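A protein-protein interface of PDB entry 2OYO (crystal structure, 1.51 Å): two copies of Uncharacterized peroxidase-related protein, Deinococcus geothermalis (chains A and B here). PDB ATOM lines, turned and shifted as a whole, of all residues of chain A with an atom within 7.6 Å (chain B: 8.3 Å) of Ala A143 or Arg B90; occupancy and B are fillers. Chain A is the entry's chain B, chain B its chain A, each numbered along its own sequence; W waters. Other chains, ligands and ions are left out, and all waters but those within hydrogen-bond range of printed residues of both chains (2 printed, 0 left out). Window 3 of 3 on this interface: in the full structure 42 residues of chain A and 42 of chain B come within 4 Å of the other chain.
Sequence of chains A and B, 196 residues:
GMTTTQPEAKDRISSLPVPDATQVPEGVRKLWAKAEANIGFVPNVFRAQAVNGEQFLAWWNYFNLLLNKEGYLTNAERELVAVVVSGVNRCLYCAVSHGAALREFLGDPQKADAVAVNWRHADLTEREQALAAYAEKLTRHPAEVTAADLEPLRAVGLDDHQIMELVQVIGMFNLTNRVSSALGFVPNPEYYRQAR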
ATOM      1  N   LYS A 137      19.236  28.742  -1.527  1.00  0.00           N
ATOM      2  CA  LYS A 137      18.857  27.410  -1.082  1.00  0.00           C
ATOM      3  C   LYS A 137      18.953  26.361  -2.165  1.00  0.00           C
ATOM      4  O   LYS A 137      19.461  25.262  -1.929  1.00  0.00           O
ATOM      5  CB  LYS A 137      17.432  27.427  -0.500  1.00  0.00           C
ATOM      6  CG  LYS A 137      17.066  26.109   0.210  1.00  0.00           C
ATOM      7  CD  LYS A 137      15.663  26.054   0.807  1.00  0.00           C
ATOM      8  CE  LYS A 137      15.378  24.658   1.349  1.00  0.00           C
ATOM      9  NZ  LYS A 137      14.091  24.677   2.146  1.00  0.00           N
ATOM     10  N   LEU A 138      18.484  26.710  -3.370  1.00  0.00           N
ATOM     11  CA  LEU A 138      18.443  25.785  -4.470  1.00  0.00           C
ATOM     12  C   LEU A 138      19.890  25.521  -4.884  1.00  0.00           C
ATOM     13  O   LEU A 138      20.236  24.442  -5.378  1.00  0.00           O
ATOM     14  CB  LEU A 138      17.559  26.301  -5.640  1.00  0.00           C
ATOM     15  CG  LEU A 138      17.348  25.295  -6.792  1.00  0.00           C
ATOM     16  CD1 LEU A 138      16.848  23.919  -6.394  1.00  0.00           C
ATOM     17  CD2 LEU A 138      16.440  25.894  -7.828  1.00  0.00           C
ATOM     18  N   ARG A 140      22.675  25.749  -2.788  1.00  0.00           N
ATOM     19  CA  ARG A 140      23.420  25.024  -1.752  1.00  0.00           C
ATOM     20  C   ARG A 140      22.827  23.681  -1.396  1.00  0.00           C
ATOM     21  O   ARG A 140      23.554  22.760  -1.093  1.00  0.00           O
ATOM     22  CB  ARG A 140      23.449  25.859  -0.489  1.00  0.00           C
ATOM     23  CG  ARG A 140      24.316  27.105  -0.618  1.00  0.00           C
ATOM     24  CD  ARG A 140      24.237  27.997   0.595  1.00  0.00           C
ATOM     25  NE  ARG A 140      24.684  27.283   1.780  1.00  0.00           N
ATOM     26  CZ  ARG A 140      24.528  27.728   3.024  1.00  0.00           C
ATOM     27  NH1 ARG A 140      23.973  28.909   3.253  1.00  0.00           N
ATOM     28  NH2 ARG A 140      24.940  26.975   4.040  1.00  0.00           N
ATOM     29  N   HIS A 141      21.499  23.593  -1.399  1.00  0.00           N
ATOM     30  CA  HIS A 141      20.761  22.422  -0.851  1.00  0.00           C
ATOM     31  C   HIS A 141      19.733  21.858  -1.821  1.00  0.00           C
ATOM     32  O   HIS A 141      18.534  21.738  -1.473  1.00  0.00           O
ATOM     33  CB  HIS A 141      20.049  22.840   0.456  1.00  0.00           C
ATOM     34  CG  HIS A 141      20.977  23.439   1.464  1.00  0.00           C
ATOM     35  ND1 HIS A 141      20.796  24.702   2.003  1.00  0.00           N
ATOM     36  CD2 HIS A 141      22.152  22.985   1.951  1.00  0.00           C
ATOM     37  CE1 HIS A 141      21.813  24.976   2.808  1.00  0.00           C
ATOM     38  NE2 HIS A 141      22.648  23.948   2.789  1.00  0.00           N
ATOM     39  N   PRO A 142      20.165  21.498  -3.022  1.00  0.00           N
ATOM     40  CA  PRO A 142      19.213  21.031  -4.031  1.00  0.00           C
ATOM     41  C   PRO A 142      18.372  19.810  -3.598  1.00  0.00           C
ATOM     42  O   PRO A 142      17.221  19.681  -4.013  1.00  0.00           O
ATOM     43  CB  PRO A 142      20.125  20.679  -5.233  1.00  0.00           C
ATOM     44  CG  PRO A 142      21.441  20.457  -4.642  1.00  0.00           C
ATOM     45  CD  PRO A 142      21.529  21.470  -3.542  1.00  0.00           C
ATOM     46  N   ALA A 143      18.952  18.932  -2.776  1.00  0.00           N
ATOM     47  CA  ALA A 143      18.268  17.740  -2.274  1.00  0.00           C
ATOM     48  C   ALA A 143      17.189  18.094  -1.293  1.00  0.00           C
ATOM     49  O   ALA A 143      16.328  17.245  -0.996  1.00  0.00           O
ATOM     50  CB  ALA A 143      19.262  16.789  -1.621  1.00  0.00           C
ATOM     51  N   GLU A 144      17.202  19.301  -0.722  1.00  0.00           N
ATOM     52  CA  GLU A 144      16.241  19.618   0.357  1.00  0.00           C
ATOM     53  C   GLU A 144      15.124  20.551  -0.022  1.00  0.00           C
ATOM     54  O   GLU A 144      14.261  20.807   0.796  1.00  0.00           O
ATOM     55  CB  GLU A 144      16.975  20.161   1.587  1.00  0.00           C
ATOM     56  CG  GLU A 144      18.110  19.234   2.037  1.00  0.00           C
ATOM     57  CD  GLU A 144      19.022  19.877   3.056  1.00  0.00           C
ATOM     58  OE1 GLU A 144      18.632  20.918   3.673  1.00  0.00           O
ATOM     59  OE2 GLU A 144      20.136  19.360   3.248  1.00  0.00           O
ATOM     60  N   VAL A 145      15.111  21.082  -1.252  1.00  0.00           N
ATOM     61  CA  VAL A 145      13.991  21.923  -1.662  1.00  0.00           C
ATOM     62  C   VAL A 145      12.746  21.088  -1.879  1.00  0.00           C
ATOM     63  O   VAL A 145      12.817  19.954  -2.316  1.00  0.00           O
ATOM     64  CB  VAL A 145      14.292  22.813  -2.912  1.00  0.00           C
ATOM     65  CG1 VAL A 145      15.363  23.814  -2.572  1.00  0.00           C
ATOM     66  CG2 VAL A 145      14.622  21.977  -4.145  1.00  0.00           C
ATOM     67  N   THR A 146      11.602  21.658  -1.561  1.00  0.00           N
ATOM     68  CA  THR A 146      10.347  20.983  -1.750  1.00  0.00           C
ATOM     69  C   THR A 146       9.315  21.964  -2.327  1.00  0.00           C
ATOM     70  O   THR A 146       9.584  23.154  -2.502  1.00  0.00           O
ATOM     71  CB  THR A 146       9.803  20.399  -0.411  1.00  0.00           C
ATOM     72  OG1 THR A 146       9.359  21.459   0.435  1.00  0.00           O
ATOM     73  CG2 THR A 146      10.872  19.544   0.334  1.00  0.00           C
ATOM     74  N   VAL B  83      24.600  10.082 -13.783  1.00  0.00           N
ATOM     75  CA  VAL B  83      24.188   9.250 -12.661  1.00  0.00           C
ATOM     76  C   VAL B  83      24.934   9.700 -11.377  1.00  0.00           C
ATOM     77  O   VAL B  83      24.321   9.825 -10.320  1.00  0.00           O
ATOM     78  CB  VAL B  83      24.344   7.712 -12.993  1.00  0.00           C
ATOM     79  CG1 VAL B  83      24.305   6.826 -11.733  1.00  0.00           C
ATOM     80  CG2 VAL B  83      23.227   7.302 -14.012  1.00  0.00           C
ATOM     81  N   VAL B  84      26.233   9.969 -11.496  1.00  0.00           N
ATOM     82  CA  VAL B  84      27.007  10.462 -10.354  1.00  0.00           C
ATOM     83  C   VAL B  84      26.474  11.799  -9.840  1.00  0.00           C
ATOM     84  O   VAL B  84      26.206  11.963  -8.631  1.00  0.00           O
ATOM     85  CB  VAL B  84      28.504  10.526 -10.659  1.00  0.00           C
ATOM     86  CG1 VAL B  84      29.272  11.263  -9.516  1.00  0.00           C
ATOM     87  CG2 VAL B  84      29.076   9.116 -10.920  1.00  0.00           C
ATOM     88  N   VAL B  85      26.307  12.767 -10.728  1.00  0.00           N
ATOM     89  CA  VAL B  85      25.837  14.096 -10.329  1.00  0.00           C
ATOM     90  C   VAL B  85      24.453  13.995  -9.741  1.00  0.00           C
ATOM     91  O   VAL B  85      24.136  14.568  -8.674  1.00  0.00           O
ATOM     92  CB  VAL B  85      25.870  15.056 -11.539  1.00  0.00           C
ATOM     93  CG1 VAL B  85      25.223  16.395 -11.165  1.00  0.00           C
ATOM     94  CG2 VAL B  85      27.326  15.223 -12.030  1.00  0.00           C
ATOM     95  N   SER B  86      23.574  13.286 -10.423  1.00  0.00           N
ATOM     96  CA  SER B  86      22.191  13.190  -9.973  1.00  0.00           C
ATOM     97  C   SER B  86      22.093  12.439  -8.636  1.00  0.00           C
ATOM     98  O   SER B  86      21.196  12.722  -7.843  1.00  0.00           O
ATOM     99  CB  SER B  86      21.282  12.527 -11.035  1.00  0.00           C
ATOM    100  OG  SER B  86      21.332  13.225 -12.237  1.00  0.00           O
ATOM    101  N   GLY B  87      22.965  11.461  -8.413  1.00  0.00           N
ATOM    102  CA  GLY B  87      23.037  10.759  -7.126  1.00  0.00           C
ATOM    103  C   GLY B  87      23.508  11.677  -6.010  1.00  0.00           C
ATOM    104  O   GLY B  87      22.915  11.708  -4.955  1.00  0.00           O
ATOM    105  N   VAL B  88      24.579  12.437  -6.241  1.00  0.00           N
ATOM    106  CA  VAL B  88      25.048  13.418  -5.226  1.00  0.00           C
ATOM    107  C   VAL B  88      23.952  14.431  -4.845  1.00  0.00           C
ATOM    108  O   VAL B  88      23.697  14.686  -3.671  1.00  0.00           O
ATOM    109  CB  VAL B  88      26.342  14.178  -5.714  1.00  0.00           C
ATOM    110  CG1 VAL B  88      26.694  15.403  -4.854  1.00  0.00           C
ATOM    111  CG2 VAL B  88      27.559  13.260  -5.810  1.00  0.00           C
ATOM    112  N   ASN B  89      23.266  14.967  -5.850  1.00  0.00           N
ATOM    113  CA  ASN B  89      22.221  15.938  -5.624  1.00  0.00           C
ATOM    114  C   ASN B  89      20.890  15.333  -5.223  1.00  0.00           C
ATOM    115  O   ASN B  89      19.991  16.073  -4.874  1.00  0.00           O
ATOM    116  CB  ASN B  89      22.033  16.832  -6.888  1.00  0.00           C
ATOM    117  CG  ASN B  89      23.210  17.788  -7.137  1.00  0.00           C
ATOM    118  OD1 ASN B  89      23.833  18.240  -6.175  1.00  0.00           O
ATOM    119  ND2 ASN B  89      23.482  18.123  -8.393  1.00  0.00           N
ATOM    120  N   ARG B  90      20.782  14.003  -5.263  1.00  0.00           N
ATOM    121  CA  ARG B  90      19.561  13.259  -4.900  1.00  0.00           C
ATOM    122  C   ARG B  90      18.362  13.793  -5.659  1.00  0.00           C
ATOM    123  O   ARG B  90      17.322  14.085  -5.087  1.00  0.00           O
ATOM    124  CB  ARG B  90      19.376  13.250  -3.358  1.00  0.00           C
ATOM    125  CG  ARG B  90      20.612  12.700  -2.646  1.00  0.00           C
ATOM    126  CD  ARG B  90      20.581  13.039  -1.149  1.00  0.00           C
ATOM    127  NE  ARG B  90      19.492  12.357  -0.510  1.00  0.00           N
ATOM    128  CZ  ARG B  90      18.955  12.727   0.653  1.00  0.00           C
ATOM    129  NH1 ARG B  90      19.408  13.801   1.295  1.00  0.00           N
ATOM    130  NH2 ARG B  90      17.936  12.031   1.144  1.00  0.00           N
ATOM    131  N   CYS B  91      18.519  13.925  -6.976  1.00  0.00           N
ATOM    132  CA  CYS B  91      17.413  14.337  -7.851  1.00  0.00           C
ATOM    133  C   CYS B  91      16.665  13.118  -8.383  1.00  0.00           C
ATOM    134  O   CYS B  91      17.218  12.336  -9.128  1.00  0.00           O
ATOM    135  CB  CYS B  91      17.913  15.148  -9.051  1.00  0.00           C
ATOM    136  SG  CYS B  91      16.572  15.608 -10.131  1.00  0.00           S
ATOM    137  N   LEU B  92      15.396  12.963  -8.046  1.00  0.00           N
ATOM    138  CA  LEU B  92      14.716  11.751  -8.453  1.00  0.00           C
ATOM    139  C   LEU B  92      14.527  11.606  -9.935  1.00  0.00           C
ATOM    140  O   LEU B  92      14.866  10.559 -10.494  1.00  0.00           O
ATOM    141  CB  LEU B  92      13.354  11.703  -7.817  1.00  0.00           C
ATOM    142  CG  LEU B  92      12.507  10.460  -8.177  1.00  0.00           C
ATOM    143  CD1 LEU B  92      12.979   9.127  -7.576  1.00  0.00           C
ATOM    144  CD2 LEU B  92      11.071  10.732  -7.785  1.00  0.00           C
ATOM    145  N   TYR B  93      14.005  12.643 -10.584  1.00  0.00           N
ATOM    146  CA  TYR B  93      13.732  12.553 -12.007  1.00  0.00           C
ATOM    147  C   TYR B  93      14.969  12.122 -12.763  1.00  0.00           C
ATOM    148  O   TYR B  93      14.934  11.170 -13.560  1.00  0.00           O
ATOM    149  CB  TYR B  93      13.139  13.848 -12.598  1.00  0.00           C
ATOM    150  CG  TYR B  93      12.660  13.623 -14.006  1.00  0.00           C
ATOM    151  CD1 TYR B  93      13.561  13.579 -15.058  1.00  0.00           C
ATOM    152  CD2 TYR B  93      11.324  13.369 -14.270  1.00  0.00           C
ATOM    153  CE1 TYR B  93      13.118  13.335 -16.370  1.00  0.00           C
ATOM    154  CE2 TYR B  93      10.864  13.128 -15.558  1.00  0.00           C
ATOM    155  CZ  TYR B  93      11.766  13.096 -16.606  1.00  0.00           C
ATOM    156  OH  TYR B  93      11.360  12.830 -17.892  1.00  0.00           O
ATOM    157  N   CYS B  94      16.060  12.833 -12.532  1.00  0.00           N
ATOM    158  CA  CYS B  94      17.317  12.611 -13.243  1.00  0.00           C
ATOM    159  C   CYS B  94      18.016  11.299 -12.882  1.00  0.00           C
ATOM    160  O   CYS B  94      18.434  10.595 -13.767  1.00  0.00           O
ATOM    161  CB  CYS B  94      18.253  13.799 -13.088  1.00  0.00           C
ATOM    162  SG  CYS B  94      17.625  15.365 -13.732  1.00  0.00           S
ATOM    163  N   ALA B  95      18.052  10.924 -11.606  1.00  0.00           N
ATOM    164  CA  ALA B  95      18.574   9.626 -11.193  1.00  0.00           C
ATOM    165  C   ALA B  95      17.877   8.455 -11.893  1.00  0.00           C
ATOM    166  O   ALA B  95      18.526   7.558 -12.408  1.00  0.00           O
ATOM    167  CB  ALA B  95      18.493   9.475  -9.655  1.00  0.00           C
ATOM    168  N   ALA B 116      24.975   4.567  -9.051  1.00  0.00           N
ATOM    169  CA  ALA B 116      23.948   5.397  -8.458  1.00  0.00           C
ATOM    170  C   ALA B 116      24.115   5.568  -6.958  1.00  0.00           C
ATOM    171  O   ALA B 116      23.775   6.620  -6.437  1.00  0.00           O
ATOM    172  CB  ALA B 116      22.581   4.865  -8.792  1.00  0.00           C
ATOM    173  N   THR B 139      30.532  19.139  -8.565  1.00  0.00           N
ATOM    174  CA  THR B 139      29.141  19.212  -8.098  1.00  0.00           C
ATOM    175  C   THR B 139      29.110  19.740  -6.670  1.00  0.00           C
ATOM    176  O   THR B 139      28.310  20.624  -6.371  1.00  0.00           O
ATOM    177  CB  THR B 139      28.398  17.835  -8.218  1.00  0.00           C
ATOM    178  OG1 THR B 139      28.315  17.487  -9.638  1.00  0.00           O
ATOM    179  CG2 THR B 139      26.982  17.879  -7.563  1.00  0.00           C
ATOM    180  N   ASN B 177      19.203  18.870 -12.386  1.00  0.00           N
ATOM    181  CA  ASN B 177      18.883  18.428 -11.010  1.00  0.00           C
ATOM    182  C   ASN B 177      18.090  19.485 -10.238  1.00  0.00           C
ATOM    183  O   ASN B 177      17.110  19.193  -9.576  1.00  0.00           O
ATOM    184  CB  ASN B 177      20.140  18.042 -10.242  1.00  0.00           C
ATOM    185  CG  ASN B 177      20.782  16.775 -10.726  1.00  0.00           C
ATOM    186  OD1 ASN B 177      20.249  16.016 -11.626  1.00  0.00           O
ATOM    187  ND2 ASN B 177      21.955  16.530 -10.190  1.00  0.00           N
ATOM    188  N   ARG B 178      18.511  20.714 -10.384  1.00  0.00           N
ATOM    189  CA  ARG B 178      17.868  21.829  -9.729  1.00  0.00           C
ATOM    190  C   ARG B 178      16.503  22.142 -10.240  1.00  0.00           C
ATOM    191  O   ARG B 178      15.597  22.264  -9.444  1.00  0.00           O
ATOM    192  CB  ARG B 178      18.788  23.053  -9.679  1.00  0.00           C
ATOM    193  CG  ARG B 178      19.922  22.842  -8.687  1.00  0.00           C
ATOM    194  CD  ARG B 178      20.911  23.981  -8.629  1.00  0.00           C
ATOM    195  NE  ARG B 178      21.889  23.708  -7.562  1.00  0.00           N
ATOM    196  CZ  ARG B 178      22.937  22.878  -7.629  1.00  0.00           C
ATOM    197  NH1 ARG B 178      23.266  22.188  -8.741  1.00  0.00           N
ATOM    198  NH2 ARG B 178      23.626  22.724  -6.525  1.00  0.00           N
ATOM    199  N   SER B 180      14.487  20.085 -11.945  1.00  0.00           N
ATOM    200  CA  SER B 180      13.655  18.877 -11.645  1.00  0.00           C
ATOM    201  C   SER B 180      13.225  18.791 -10.164  1.00  0.00           C
ATOM    202  O   SER B 180      12.069  18.543  -9.825  1.00  0.00           O
ATOM    203  CB  SER B 180      14.390  17.598 -12.050  1.00  0.00           C
ATOM    204  OG  SER B 180      14.533  17.619 -13.444  1.00  0.00           O
ATOM    205  N   SER B 181      14.173  19.007  -9.276  1.00  0.00           N
ATOM    206  CA  SER B 181      13.892  18.967  -7.827  1.00  0.00           C
ATOM    207  C   SER B 181      13.031  20.140  -7.353  1.00  0.00           C
ATOM    208  O   SER B 181      12.044  19.958  -6.637  1.00  0.00           O
ATOM    209  CB  SER B 181      15.208  18.867  -7.046  1.00  0.00           C
ATOM    210  OG  SER B 181      15.853  17.647  -7.362  1.00  0.00           O
ATOM    211  N   ALA B 182      13.361  21.347  -7.806  1.00  0.00           N
ATOM    212  CA  ALA B 182      12.606  22.523  -7.421  1.00  0.00           C
ATOM    213  C   ALA B 182      11.153  22.378  -7.744  1.00  0.00           C
ATOM    214  O   ALA B 182      10.312  22.821  -7.007  1.00  0.00           O
ATOM    215  CB  ALA B 182      13.174  23.764  -8.095  1.00  0.00           C
HETATM  216  O   HOH W   1      18.543  17.828  -6.587  1.00  0.00           O
HETATM  217  O   HOH W   2      10.940  24.110  -4.716  1.00  0.00           O
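O of Leu A138 lies within hydrogen-bond range of NE of Arg B178 (2.8 Å).
The side-chain amide nitrogen of Asn B177 lies close to the side-chain amide nitrogen of Asn B89 (2.8 Å). SG of Cys B91 sits at hydrogen-bond distance from OG of Ser B181 (3.5 Å). OG of Ser B181 lies within hydrogen-bond range of O of Asn B177.
Among the printed residues, pairs that only touch across the chains: Leu A138 with Ala B182 (3.9 Å), Pro A142 with Asn B89 (3.6 Å), Pro A142 with Arg B178 (3.7 Å), Pro A142 with Ser B181 (3.7 Å), Ala A143 with Asn B89 (3.4 Å), Ala A143 with Arg B90 (3.9 Å) and Val A145 with Ala B182 (3.9 Å).
Of chain B, only Asn B89 (3.4 Å) and Arg B90 (3.9 Å) come within 4 Å of Ala A143. Of the printed residues of chain B, Val A145 touches Ala B182. Of the printed residues of chain A, Asn B89 touches Pro A142 (3.6 Å) and Ala A143 (3.4 Å). Arg B90 touches just one residue of chain A: Ala A143. Leu B92 touches none of the printed residues of chain A. Of the printed residues of chain A, Ala B182 touches Leu A138 and Val A145. The nearest residue of chain B that does not touch Ala A143 is Val B88 (5.3 Å). The nearest residue of chain A that does not touch Arg B90 is Glu A144 (5.6 Å). The nearest printed residue of chain B that does not touch Val A145 is Ser B181 (4.02 Å).
Hydrophobic or aromatic side chains of chain B within 4 Å of the printed part of chain A: Ala B182. Printed residues of chain A that touch a printed residue of chain B: Leu A138, Pro A142, Ala A143 and Val A145. Hydrophobic or aromatic side chains of chain A within 4 Å of the printed part of chain B: Leu A138, Pro A142, Ala A143 and Val A145. Among the printed residues, no Asp or Glu carboxylate lies within 4 Å of a Lys or Arg side-chain nitrogen of the other chain.
No position is printed for both chains. Of the 8 pairs that touch across the chains among the printed residues, none has its exchanged pair printed and touching as well.
Water W2 bridges O of Ala B182 (2.7 Å) and O of Thr A146 (2.8 Å). Water W1 lies within hydrogen-bond range of the side-chain hydroxyl (OG) of Ser B181 (2.8 Å), the backbone carbonyl oxygen (O) of Asn B89 (2.8 Å) and the backbone carbonyl oxygen (O) of Pro A142 (3.4 Å).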
